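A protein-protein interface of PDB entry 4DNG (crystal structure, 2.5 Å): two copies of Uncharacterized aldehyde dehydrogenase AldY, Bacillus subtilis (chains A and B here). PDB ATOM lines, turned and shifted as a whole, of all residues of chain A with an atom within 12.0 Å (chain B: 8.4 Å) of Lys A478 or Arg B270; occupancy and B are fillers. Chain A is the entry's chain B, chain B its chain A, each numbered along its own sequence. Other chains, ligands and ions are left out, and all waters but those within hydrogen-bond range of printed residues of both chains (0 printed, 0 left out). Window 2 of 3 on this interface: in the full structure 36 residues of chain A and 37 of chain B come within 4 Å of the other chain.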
ATOM      1  N   GLU A 127      -5.675  -2.110  -0.002  1.00  0.00           N
ATOM      2  CA  GLU A 127      -4.747  -2.290   1.119  1.00  0.00           C
ATOM      3  C   GLU A 127      -4.484  -3.759   1.442  1.00  0.00           C
ATOM      4  O   GLU A 127      -3.385  -4.129   1.859  1.00  0.00           O
ATOM      5  CB  GLU A 127      -5.259  -1.560   2.365  1.00  0.00           C
ATOM      6  CG  GLU A 127      -5.630  -0.092   2.148  1.00  0.00           C
ATOM      7  CD  GLU A 127      -4.447   0.830   1.841  1.00  0.00           C
ATOM      8  OE1 GLU A 127      -4.680   2.050   1.669  1.00  0.00           O
ATOM      9  OE2 GLU A 127      -3.289   0.358   1.771  1.00  0.00           O
ATOM     10  N   GLU A 133       0.891 -11.320   4.807  1.00  0.00           N
ATOM     11  CA  GLU A 133       1.997 -10.683   4.101  1.00  0.00           C
ATOM     12  C   GLU A 133       2.316 -11.373   2.771  1.00  0.00           C
ATOM     13  O   GLU A 133       3.262 -11.008   2.066  1.00  0.00           O
ATOM     14  CB  GLU A 133       3.236 -10.604   4.997  1.00  0.00           C
ATOM     15  CG  GLU A 133       4.016  -9.303   4.856  1.00  0.00           C
ATOM     16  CD  GLU A 133       3.387  -8.131   5.599  1.00  0.00           C
ATOM     17  OE1 GLU A 133       2.185  -8.187   5.954  1.00  0.00           O
ATOM     18  OE2 GLU A 133       4.106  -7.138   5.828  1.00  0.00           O
ATOM     19  N   GLY A 134       1.537 -12.403   2.461  1.00  0.00           N
ATOM     20  CA  GLY A 134       1.344 -12.848   1.087  1.00  0.00           C
ATOM     21  C   GLY A 134      -0.018 -12.299   0.680  1.00  0.00           C
ATOM     22  O   GLY A 134      -0.402 -12.346  -0.489  1.00  0.00           O
ATOM     23  N   LYS A 135      -0.730 -11.761   1.672  1.00  0.00           N
ATOM     24  CA  LYS A 135      -2.106 -11.291   1.532  1.00  0.00           C
ATOM     25  C   LYS A 135      -2.231  -9.889   0.948  1.00  0.00           C
ATOM     26  O   LYS A 135      -1.284  -9.102   0.968  1.00  0.00           O
ATOM     27  CB  LYS A 135      -2.817 -11.322   2.893  1.00  0.00           C
ATOM     28  CG  LYS A 135      -3.182 -12.715   3.368  1.00  0.00           C
ATOM     29  CD  LYS A 135      -4.324 -12.696   4.366  1.00  0.00           C
ATOM     30  CE  LYS A 135      -5.057 -14.030   4.365  1.00  0.00           C
ATOM     31  NZ  LYS A 135      -6.033 -14.159   3.242  1.00  0.00           N
ATOM     32  N   THR A 136      -3.416  -9.594   0.424  1.00  0.00           N
ATOM     33  CA  THR A 136      -3.793  -8.234   0.061  1.00  0.00           C
ATOM     34  C   THR A 136      -5.276  -7.999   0.332  1.00  0.00           C
ATOM     35  O   THR A 136      -6.120  -8.876   0.120  1.00  0.00           O
ATOM     36  CB  THR A 136      -3.438  -7.867  -1.394  1.00  0.00           C
ATOM     37  OG1 THR A 136      -4.174  -6.698  -1.777  1.00  0.00           O
ATOM     38  CG2 THR A 136      -3.753  -9.011  -2.352  1.00  0.00           C
ATOM     39  N   ASN A 137      -5.586  -6.801   0.797  1.00  0.00           N
ATOM     40  CA  ASN A 137      -6.886  -6.547   1.338  1.00  0.00           C
ATOM     41  C   ASN A 137      -7.605  -5.458   0.579  1.00  0.00           C
ATOM     42  O   ASN A 137      -7.287  -4.276   0.707  1.00  0.00           O
ATOM     43  CB  ASN A 137      -6.761  -6.243   2.826  1.00  0.00           C
ATOM     44  CG  ASN A 137      -6.111  -7.384   3.595  1.00  0.00           C
ATOM     45  OD1 ASN A 137      -6.770  -8.356   3.950  1.00  0.00           O
ATOM     46  ND2 ASN A 137      -4.815  -7.270   3.854  1.00  0.00           N
ATOM     47  N   LYS A 138      -8.577  -5.878  -0.223  1.00  0.00           N
ATOM     48  CA  LYS A 138      -9.385  -4.955  -1.003  1.00  0.00           C
ATOM     49  C   LYS A 138     -10.609  -4.575  -0.189  1.00  0.00           C
ATOM     50  O   LYS A 138     -11.419  -5.440   0.173  1.00  0.00           O
ATOM     51  CB  LYS A 138      -9.818  -5.587  -2.335  1.00  0.00           C
ATOM     52  CG  LYS A 138      -8.731  -6.304  -3.130  1.00  0.00           C
ATOM     53  CD  LYS A 138      -8.050  -5.408  -4.162  1.00  0.00           C
ATOM     54  CE  LYS A 138      -6.631  -5.038  -3.747  1.00  0.00           C
ATOM     55  NZ  LYS A 138      -5.805  -4.508  -4.872  1.00  0.00           N
ATOM     56  N   ILE A 474     -12.360  -8.140   0.992  1.00  0.00           N
ATOM     57  CA  ILE A 474     -11.931  -9.355   0.320  1.00  0.00           C
ATOM     58  C   ILE A 474     -10.432  -9.494   0.557  1.00  0.00           C
ATOM     59  O   ILE A 474      -9.661  -8.600   0.193  1.00  0.00           O
ATOM     60  CB  ILE A 474     -12.219  -9.319  -1.204  1.00  0.00           C
ATOM     61  CG1 ILE A 474     -13.705  -9.081  -1.481  1.00  0.00           C
ATOM     62  CG2 ILE A 474     -11.782 -10.619  -1.867  1.00  0.00           C
ATOM     63  CD1 ILE A 474     -13.989  -8.552  -2.870  1.00  0.00           C
ATOM     64  N   SER A 475     -10.034 -10.600   1.185  1.00  0.00           N
ATOM     65  CA  SER A 475      -8.618 -10.951   1.370  1.00  0.00           C
ATOM     66  C   SER A 475      -8.171 -11.924   0.306  1.00  0.00           C
ATOM     67  O   SER A 475      -8.778 -12.973   0.131  1.00  0.00           O
ATOM     68  CB  SER A 475      -8.382 -11.593   2.731  1.00  0.00           C
ATOM     69  OG  SER A 475      -7.647 -10.721   3.561  1.00  0.00           O
ATOM     70  N   ILE A 476      -7.096 -11.578  -0.389  1.00  0.00           N
ATOM     71  CA  ILE A 476      -6.621 -12.355  -1.518  1.00  0.00           C
ATOM     72  C   ILE A 476      -5.215 -12.896  -1.222  1.00  0.00           C
ATOM     73  O   ILE A 476      -4.324 -12.137  -0.836  1.00  0.00           O
ATOM     74  CB  ILE A 476      -6.655 -11.508  -2.811  1.00  0.00           C
ATOM     75  CG1 ILE A 476      -8.066 -10.971  -3.057  1.00  0.00           C
ATOM     76  CG2 ILE A 476      -6.206 -12.331  -4.007  1.00  0.00           C
ATOM     77  CD1 ILE A 476      -8.165  -9.915  -4.136  1.00  0.00           C
ATOM     78  N   GLN A 477      -5.031 -14.206  -1.393  1.00  0.00           N
ATOM     79  CA  GLN A 477      -3.757 -14.876  -1.074  1.00  0.00           C
ATOM     80  C   GLN A 477      -2.875 -15.199  -2.309  1.00  0.00           C
ATOM     81  O   GLN A 477      -3.375 -15.262  -3.438  1.00  0.00           O
ATOM     82  CB  GLN A 477      -4.032 -16.144  -0.250  1.00  0.00           C
ATOM     83  CG  GLN A 477      -2.799 -16.809   0.359  1.00  0.00           C
ATOM     84  CD  GLN A 477      -1.972 -15.864   1.213  1.00  0.00           C
ATOM     85  OE1 GLN A 477      -2.512 -15.114   2.031  1.00  0.00           O
ATOM     86  NE2 GLN A 477      -0.650 -15.893   1.025  1.00  0.00           N
ATOM     87  N   LYS A 478      -1.570 -15.385  -2.072  1.00  0.00           N
ATOM     88  CA  LYS A 478      -0.602 -15.843  -3.090  1.00  0.00           C
ATOM     89  C   LYS A 478      -0.513 -17.367  -3.155  1.00  0.00           C
ATOM     90  O   LYS A 478       0.500 -17.967  -2.716  1.00  0.00           O
ATOM     91  CB  LYS A 478       0.793 -15.275  -2.807  1.00  0.00           C
ATOM     92  CG  LYS A 478       0.895 -13.763  -2.875  1.00  0.00           C
ATOM     93  CD  LYS A 478       2.303 -13.297  -2.534  1.00  0.00           C
ATOM     94  CE  LYS A 478       2.364 -11.782  -2.386  1.00  0.00           C
ATOM     95  NZ  LYS A 478       3.765 -11.290  -2.252  1.00  0.00           N
ATOM     96  N   PHE B 260     -17.920 -22.477   2.403  1.00  0.00           N
ATOM     97  CA  PHE B 260     -16.625 -22.703   1.820  1.00  0.00           C
ATOM     98  C   PHE B 260     -16.974 -23.130   0.404  1.00  0.00           C
ATOM     99  O   PHE B 260     -17.566 -24.196   0.201  1.00  0.00           O
ATOM    100  CB  PHE B 260     -15.979 -23.864   2.579  1.00  0.00           C
ATOM    101  CG  PHE B 260     -14.505 -24.027   2.356  1.00  0.00           C
ATOM    102  CD1 PHE B 260     -13.587 -23.271   3.084  1.00  0.00           C
ATOM    103  CD2 PHE B 260     -14.030 -24.988   1.475  1.00  0.00           C
ATOM    104  CE1 PHE B 260     -12.221 -23.431   2.898  1.00  0.00           C
ATOM    105  CE2 PHE B 260     -12.661 -25.165   1.293  1.00  0.00           C
ATOM    106  CZ  PHE B 260     -11.758 -24.386   2.006  1.00  0.00           C
ATOM    107  N   VAL B 262     -15.684 -24.116  -3.415  1.00  0.00           N
ATOM    108  CA  VAL B 262     -14.535 -24.679  -4.120  1.00  0.00           C
ATOM    109  C   VAL B 262     -14.894 -24.808  -5.598  1.00  0.00           C
ATOM    110  O   VAL B 262     -15.590 -25.746  -6.016  1.00  0.00           O
ATOM    111  CB  VAL B 262     -14.146 -26.057  -3.528  1.00  0.00           C
ATOM    112  CG1 VAL B 262     -13.093 -26.757  -4.387  1.00  0.00           C
ATOM    113  CG2 VAL B 262     -13.669 -25.910  -2.094  1.00  0.00           C
ATOM    114  N   ALA B 266     -10.301 -24.319  -9.059  1.00  0.00           N
ATOM    115  CA  ALA B 266      -9.529 -24.393  -7.804  1.00  0.00           C
ATOM    116  C   ALA B 266      -8.428 -25.447  -7.775  1.00  0.00           C
ATOM    117  O   ALA B 266      -8.529 -26.499  -8.415  1.00  0.00           O
ATOM    118  CB  ALA B 266     -10.456 -24.626  -6.632  1.00  0.00           C
ATOM    119  N   ASP B 267      -7.373 -25.158  -7.020  1.00  0.00           N
ATOM    120  CA  ASP B 267      -6.399 -26.172  -6.669  1.00  0.00           C
ATOM    121  C   ASP B 267      -7.059 -26.998  -5.575  1.00  0.00           C
ATOM    122  O   ASP B 267      -7.295 -26.484  -4.483  1.00  0.00           O
ATOM    123  CB  ASP B 267      -5.115 -25.516  -6.155  1.00  0.00           C
ATOM    124  CG  ASP B 267      -4.119 -26.520  -5.575  1.00  0.00           C
ATOM    125  OD1 ASP B 267      -4.532 -27.508  -4.918  1.00  0.00           O
ATOM    126  OD2 ASP B 267      -2.906 -26.301  -5.756  1.00  0.00           O
ATOM    127  N   VAL B 268      -7.370 -28.257  -5.869  1.00  0.00           N
ATOM    128  CA  VAL B 268      -8.091 -29.115  -4.927  1.00  0.00           C
ATOM    129  C   VAL B 268      -7.278 -29.346  -3.650  1.00  0.00           C
ATOM    130  O   VAL B 268      -7.785 -29.139  -2.528  1.00  0.00           O
ATOM    131  CB  VAL B 268      -8.515 -30.452  -5.573  1.00  0.00           C
ATOM    132  CG1 VAL B 268      -9.053 -31.439  -4.543  1.00  0.00           C
ATOM    133  CG2 VAL B 268      -9.563 -30.196  -6.631  1.00  0.00           C
ATOM    134  N   ASP B 269      -6.015 -29.731  -3.830  1.00  0.00           N
ATOM    135  CA  ASP B 269      -5.132 -30.045  -2.708  1.00  0.00           C
ATOM    136  C   ASP B 269      -5.012 -28.907  -1.682  1.00  0.00           C
ATOM    137  O   ASP B 269      -5.110 -29.133  -0.473  1.00  0.00           O
ATOM    138  CB  ASP B 269      -3.757 -30.461  -3.222  1.00  0.00           C
ATOM    139  CG  ASP B 269      -3.210 -31.656  -2.486  1.00  0.00           C
ATOM    140  OD1 ASP B 269      -3.326 -32.777  -3.031  1.00  0.00           O
ATOM    141  OD2 ASP B 269      -2.692 -31.477  -1.356  1.00  0.00           O
ATOM    142  N   ARG B 270      -4.807 -27.689  -2.170  1.00  0.00           N
ATOM    143  CA  ARG B 270      -4.860 -26.498  -1.330  1.00  0.00           C
ATOM    144  C   ARG B 270      -6.209 -26.421  -0.596  1.00  0.00           C
ATOM    145  O   ARG B 270      -6.234 -26.177   0.614  1.00  0.00           O
ATOM    146  CB  ARG B 270      -4.626 -25.254  -2.194  1.00  0.00           C
ATOM    147  CG  ARG B 270      -4.181 -23.993  -1.463  1.00  0.00           C
ATOM    148  CD  ARG B 270      -3.517 -23.037  -2.453  1.00  0.00           C
ATOM    149  NE  ARG B 270      -3.503 -21.644  -2.002  1.00  0.00           N
ATOM    150  CZ  ARG B 270      -2.404 -20.926  -1.768  1.00  0.00           C
ATOM    151  NH1 ARG B 270      -2.519 -19.668  -1.365  1.00  0.00           N
ATOM    152  NH2 ARG B 270      -1.193 -21.451  -1.941  1.00  0.00           N
ATOM    153  N   ALA B 271      -7.304 -26.677  -1.327  1.00  0.00           N
ATOM    154  CA  ALA B 271      -8.688 -26.547  -0.819  1.00  0.00           C
ATOM    155  C   ALA B 271      -9.070 -27.600   0.224  1.00  0.00           C
ATOM    156  O   ALA B 271      -9.700 -27.278   1.234  1.00  0.00           O
ATOM    157  CB  ALA B 271      -9.702 -26.556  -1.966  1.00  0.00           C
ATOM    158  N   VAL B 272      -8.700 -28.851  -0.020  1.00  0.00           N
ATOM    159  CA  VAL B 272      -8.866 -29.885   0.995  1.00  0.00           C
ATOM    160  C   VAL B 272      -8.124 -29.474   2.269  1.00  0.00           C
ATOM    161  O   VAL B 272      -8.717 -29.420   3.344  1.00  0.00           O
ATOM    162  CB  VAL B 272      -8.344 -31.243   0.509  1.00  0.00           C
ATOM    163  CG1 VAL B 272      -8.519 -32.296   1.600  1.00  0.00           C
ATOM    164  CG2 VAL B 272      -9.032 -31.653  -0.785  1.00  0.00           C
ATOM    165  N   ASP B 273      -6.839 -29.154   2.123  1.00  0.00           N
ATOM    166  CA  ASP B 273      -5.984 -28.724   3.236  1.00  0.00           C
ATOM    167  C   ASP B 273      -6.579 -27.558   4.019  1.00  0.00           C
ATOM    168  O   ASP B 273      -6.753 -27.651   5.236  1.00  0.00           O
ATOM    169  CB  ASP B 273      -4.574 -28.349   2.747  1.00  0.00           C
ATOM    170  CG  ASP B 273      -3.669 -29.557   2.568  1.00  0.00           C
ATOM    171  OD1 ASP B 273      -3.767 -30.514   3.367  1.00  0.00           O
ATOM    172  OD2 ASP B 273      -2.846 -29.537   1.628  1.00  0.00           O
ATOM    173  N   ALA B 274      -6.895 -26.472   3.317  1.00  0.00           N
ATOM    174  CA  ALA B 274      -7.485 -25.298   3.950  1.00  0.00           C
ATOM    175  C   ALA B 274      -8.832 -25.602   4.624  1.00  0.00           C
ATOM    176  O   ALA B 274      -9.173 -24.964   5.614  1.00  0.00           O
ATOM    177  CB  ALA B 274      -7.619 -24.161   2.952  1.00  0.00           C
ATOM    178  N   ALA B 275      -9.584 -26.575   4.099  1.00  0.00           N
ATOM    179  CA  ALA B 275     -10.839 -27.013   4.728  1.00  0.00           C
ATOM    180  C   ALA B 275     -10.620 -27.834   6.006  1.00  0.00           C
ATOM    181  O   ALA B 275     -11.457 -27.819   6.906  1.00  0.00           O
ATOM    182  CB  ALA B 275     -11.699 -27.788   3.746  1.00  0.00           C
ATOM    183  N   ILE B 276      -9.510 -28.563   6.082  1.00  0.00           N
ATOM    184  CA  ILE B 276      -9.170 -29.299   7.303  1.00  0.00           C
ATOM    185  C   ILE B 276      -8.755 -28.358   8.445  1.00  0.00           C
ATOM    186  O   ILE B 276      -9.281 -28.470   9.553  1.00  0.00           O
ATOM    187  CB  ILE B 276      -8.101 -30.385   7.043  1.00  0.00           C
ATOM    188  CG1 ILE B 276      -8.772 -31.731   6.782  1.00  0.00           C
ATOM    189  CG2 ILE B 276      -7.168 -30.551   8.237  1.00  0.00           C
ATOM    190  CD1 ILE B 276      -9.121 -31.966   5.341  1.00  0.00           C
ATOM    191  N   PHE B 277      -7.819 -27.443   8.162  1.00  0.00           N
ATOM    192  CA  PHE B 277      -7.321 -26.466   9.133  1.00  0.00           C
ATOM    193  C   PHE B 277      -8.484 -25.673   9.723  1.00  0.00           C
ATOM    194  O   PHE B 277      -8.622 -25.599  10.936  1.00  0.00           O
ATOM    195  CB  PHE B 277      -6.274 -25.525   8.486  1.00  0.00           C
ATOM    196  CG  PHE B 277      -5.577 -24.589   9.465  1.00  0.00           C
ATOM    197  CD1 PHE B 277      -4.439 -25.003  10.171  1.00  0.00           C
ATOM    198  CD2 PHE B 277      -6.039 -23.284   9.664  1.00  0.00           C
ATOM    199  CE1 PHE B 277      -3.792 -24.148  11.064  1.00  0.00           C
ATOM    200  CE2 PHE B 277      -5.395 -22.430  10.554  1.00  0.00           C
ATOM    201  CZ  PHE B 277      -4.271 -22.861  11.253  1.00  0.00           C
ATOM    202  N   GLU B 302     -12.922 -35.912  -6.528  1.00  0.00           N
ATOM    203  CA  GLU B 302     -11.534 -35.744  -6.091  1.00  0.00           C
ATOM    204  C   GLU B 302     -11.430 -35.107  -4.701  1.00  0.00           C
ATOM    205  O   GLU B 302     -10.637 -35.564  -3.867  1.00  0.00           O
ATOM    206  CB  GLU B 302     -10.740 -34.928  -7.121  1.00  0.00           C
ATOM    207  CG  GLU B 302      -9.344 -34.496  -6.677  1.00  0.00           C
ATOM    208  CD  GLU B 302      -8.535 -33.817  -7.781  1.00  0.00           C
ATOM    209  OE1 GLU B 302      -9.010 -33.723  -8.939  1.00  0.00           O
ATOM    210  OE2 GLU B 302      -7.401 -33.377  -7.498  1.00  0.00           O
ATOM    211  N   PHE B 303     -12.223 -34.058  -4.460  1.00  0.00           N
ATOM    212  CA  PHE B 303     -12.228 -33.380  -3.163  1.00  0.00           C
ATOM    213  C   PHE B 303     -12.709 -34.305  -2.046  1.00  0.00           C
ATOM    214  O   PHE B 303     -12.117 -34.303  -0.960  1.00  0.00           O
ATOM    215  CB  PHE B 303     -13.085 -32.099  -3.183  1.00  0.00           C
ATOM    216  CG  PHE B 303     -13.050 -31.311  -1.886  1.00  0.00           C
ATOM    217  CD1 PHE B 303     -13.856 -31.678  -0.799  1.00  0.00           C
ATOM    218  CD2 PHE B 303     -12.214 -30.198  -1.751  1.00  0.00           C
ATOM    219  CE1 PHE B 303     -13.823 -30.958   0.390  1.00  0.00           C
ATOM    220  CE2 PHE B 303     -12.180 -29.468  -0.571  1.00  0.00           C
ATOM    221  CZ  PHE B 303     -12.979 -29.849   0.502  1.00  0.00           C
ATOM    222  N   LYS B 306     -10.090 -37.137  -1.052  1.00  0.00           N
ATOM    223  CA  LYS B 306      -8.978 -36.505  -0.345  1.00  0.00           C
ATOM    224  C   LYS B 306      -9.366 -35.981   1.035  1.00  0.00           C
ATOM    225  O   LYS B 306      -8.639 -36.206   2.010  1.00  0.00           O
ATOM    226  CB  LYS B 306      -8.366 -35.385  -1.191  1.00  0.00           C
ATOM    227  CG  LYS B 306      -7.223 -35.858  -2.063  1.00  0.00           C
ATOM    228  CD  LYS B 306      -7.033 -34.978  -3.282  1.00  0.00           C
ATOM    229  CE  LYS B 306      -6.606 -35.842  -4.456  1.00  0.00           C
ATOM    230  NZ  LYS B 306      -6.399 -35.022  -5.673  1.00  0.00           N
ATOM    231  N   PHE B 414     -12.518 -20.623  -3.401  1.00  0.00           N
ATOM    232  CA  PHE B 414     -11.288 -21.211  -3.945  1.00  0.00           C
ATOM    233  C   PHE B 414     -11.362 -21.347  -5.447  1.00  0.00           C
ATOM    234  O   PHE B 414     -12.174 -22.095  -5.996  1.00  0.00           O
ATOM    235  CB  PHE B 414     -10.931 -22.541  -3.262  1.00  0.00           C
ATOM    236  CG  PHE B 414     -10.225 -22.364  -1.945  1.00  0.00           C
ATOM    237  CD1 PHE B 414     -10.921 -21.923  -0.820  1.00  0.00           C
ATOM    238  CD2 PHE B 414      -8.861 -22.611  -1.830  1.00  0.00           C
ATOM    239  CE1 PHE B 414     -10.276 -21.740   0.398  1.00  0.00           C
ATOM    240  CE2 PHE B 414      -8.207 -22.436  -0.615  1.00  0.00           C
ATOM    241  CZ  PHE B 414      -8.916 -21.998   0.499  1.00  0.00           C
ATOM    242  N   THR B 415     -10.509 -20.583  -6.102  1.00  0.00           N
ATOM    243  CA  THR B 415     -10.463 -20.547  -7.538  1.00  0.00           C
ATOM    244  C   THR B 415      -9.049 -20.223  -7.958  1.00  0.00           C
ATOM    245  O   THR B 415      -8.319 -19.526  -7.246  1.00  0.00           O
ATOM    246  CB  THR B 415     -11.441 -19.505  -8.135  1.00  0.00           C
ATOM    247  OG1 THR B 415     -11.104 -19.264  -9.518  1.00  0.00           O
ATOM    248  CG2 THR B 415     -11.370 -18.192  -7.373  1.00  0.00           C
ATOM    249  N   LEU B 418      -7.907 -15.404  -9.929  1.00  0.00           N
ATOM    250  CA  LEU B 418      -7.967 -14.395  -8.855  1.00  0.00           C
ATOM    251  C   LEU B 418      -8.871 -13.190  -9.163  1.00  0.00           C
ATOM    252  O   LEU B 418      -9.444 -12.593  -8.245  1.00  0.00           O
ATOM    253  CB  LEU B 418      -6.561 -13.926  -8.452  1.00  0.00           C
ATOM    254  CG  LEU B 418      -5.583 -14.931  -7.830  1.00  0.00           C
ATOM    255  CD1 LEU B 418      -4.279 -14.221  -7.499  1.00  0.00           C
ATOM    256  CD2 LEU B 418      -6.154 -15.624  -6.597  1.00  0.00           C
ATOM    257  N   VAL B 435     -10.198 -15.207  -0.577  1.00  0.00           N
ATOM    258  CA  VAL B 435      -9.990 -16.036  -1.743  1.00  0.00           C
ATOM    259  C   VAL B 435      -8.786 -16.914  -1.494  1.00  0.00           C
ATOM    260  O   VAL B 435      -7.698 -16.431  -1.272  1.00  0.00           O
ATOM    261  CB  VAL B 435      -9.747 -15.200  -2.997  1.00  0.00           C
ATOM    262  CG1 VAL B 435     -11.028 -14.560  -3.461  1.00  0.00           C
ATOM    263  CG2 VAL B 435      -8.700 -14.147  -2.731  1.00  0.00           C
ATOM    264  N   ASN B 436      -8.989 -18.214  -1.554  1.00  0.00           N
ATOM    265  CA  ASN B 436      -7.909 -19.141  -1.308  1.00  0.00           C
ATOM    266  C   ASN B 436      -7.188 -18.986   0.020  1.00  0.00           C
ATOM    267  O   ASN B 436      -5.980 -18.952   0.046  1.00  0.00           O
ATOM    268  CB  ASN B 436      -6.901 -19.075  -2.445  1.00  0.00           C
ATOM    269  CG  ASN B 436      -7.522 -19.373  -3.791  1.00  0.00           C
ATOM    270  OD1 ASN B 436      -8.380 -20.236  -3.916  1.00  0.00           O
ATOM    271  ND2 ASN B 436      -7.080 -18.659  -4.809  1.00  0.00           N
ATOM    272  N   ASP B 437      -7.923 -18.863   1.118  1.00  0.00           N
ATOM    273  CA  ASP B 437      -7.325 -18.887   2.462  1.00  0.00           C
ATOM    274  C   ASP B 437      -8.258 -19.299   3.599  1.00  0.00           C
ATOM    275  O   ASP B 437      -9.453 -19.451   3.414  1.00  0.00           O
ATOM    276  CB  ASP B 437      -6.639 -17.582   2.831  1.00  0.00           C
ATOM    277  CG  ASP B 437      -5.937 -17.668   4.170  1.00  0.00           C
ATOM    278  OD1 ASP B 437      -4.718 -17.895   4.194  1.00  0.00           O
ATOM    279  OD2 ASP B 437      -6.611 -17.528   5.204  1.00  0.00           O
ATOM    280  N   GLN B 438      -7.689 -19.512   4.777  1.00  0.00           N
ATOM    281  CA  GLN B 438      -8.479 -19.868   5.941  1.00  0.00           C
ATOM    282  C   GLN B 438      -9.326 -21.062   5.593  1.00  0.00           C
ATOM    283  O   GLN B 438      -9.433 -21.987   6.376  1.00  0.00           O
ATOM    284  CB  GLN B 438      -9.388 -18.713   6.359  1.00  0.00           C
ATOM    285  CG  GLN B 438      -8.718 -17.673   7.240  1.00  0.00           C
ATOM    286  CD  GLN B 438      -9.317 -17.588   8.633  1.00  0.00           C
ATOM    287  OE1 GLN B 438     -10.529 -17.667   8.809  1.00  0.00           O
ATOM    288  NE2 GLN B 438      -8.463 -17.416   9.629  1.00  0.00           N
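The backbone carbonyl oxygen (O) of Ser A475 is in hydrogen-bond range of the backbone NH (N) of Val B435 (2.7 Å).
O of Val B435 sits at hydrogen-bond distance from N of Gln A477.
OD2 of Asp B437 lies within salt-bridge range of NZ of Lys A135.
N of Ile A476 sits at hydrogen-bond distance from O of Thr A136, at 2.9 Å.
The side-chain amide nitrogen (ND2) of Asn B436 lies within hydrogen-bond range of the backbone carbonyl oxygen (O) of Thr B415 (2.9 Å).
The side-chain amide oxygen (OD1) of Asn A137 is in hydrogen-bond range of the side-chain hydroxyl (OG) of Ser A475, 2.6 Å away.
N of Arg B270 is in hydrogen-bond range of OD1 of Asp B267, 2.8 Å away.
Among the printed residues, pairs that only touch across the chains: Ile A476 with Val B435 (3.0 Å), Gln A477 with Arg B270 (3.4 Å), Gln A477 with Asn B436 (3.4 Å) and Lys A478 with Arg B270 (3.5 Å).
Of chain B, only Arg B270 comes within 4 Å of Lys A478.
Arg B270 touches two residues of chain A.
Of chain B, only Arg B270, Val B435 and Asn B436 come within 4 Å of Gln A477.
No residue of chain A comes within 4 Å of Val B268.
No residue of chain A comes within 4 Å of Asp B273.
No residue of chain A comes within 4 Å of Ala B274.
Asn B436 touches just one residue of chain A: Gln A477 (3.4 Å).
Printed residues of chain A within 4 Å of Val B435: Ser A475 (2.7 Å), Ile A476 (3.0 Å) and Gln A477 (3.5 Å).
Of the printed residues of chain A, Asp B437 touches Lys A135 (3.5 Å).
Printed residues of chain B within 4 Å of Ile A476: Val B435.
Of the printed residues of chain B, Lys A135 touches Asp B437 (3.5 Å).
Printed residues of chain B within 4 Å of Ser A475: Val B435 (2.7 Å).
Ile A474 touches none of the printed residues of chain B.
The nearest residue of chain A that does not touch Arg B270 is Ile A476 (7.3 Å).
Hydrophobic or aromatic side chains of chain B that line the printed part of chain A: Val B435.
Of the 12 printed residues of chain A, 5 touch a printed residue of chain B.
Among the printed residues, 7 pairs touch across the chains.
Among the printed residues, Asp or Glu carboxylates within 4 Å of a Lys or Arg side-chain nitrogen of the other chain: Lys A135 with Asp B437 (3.9 Å).
No position is printed for both chains.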
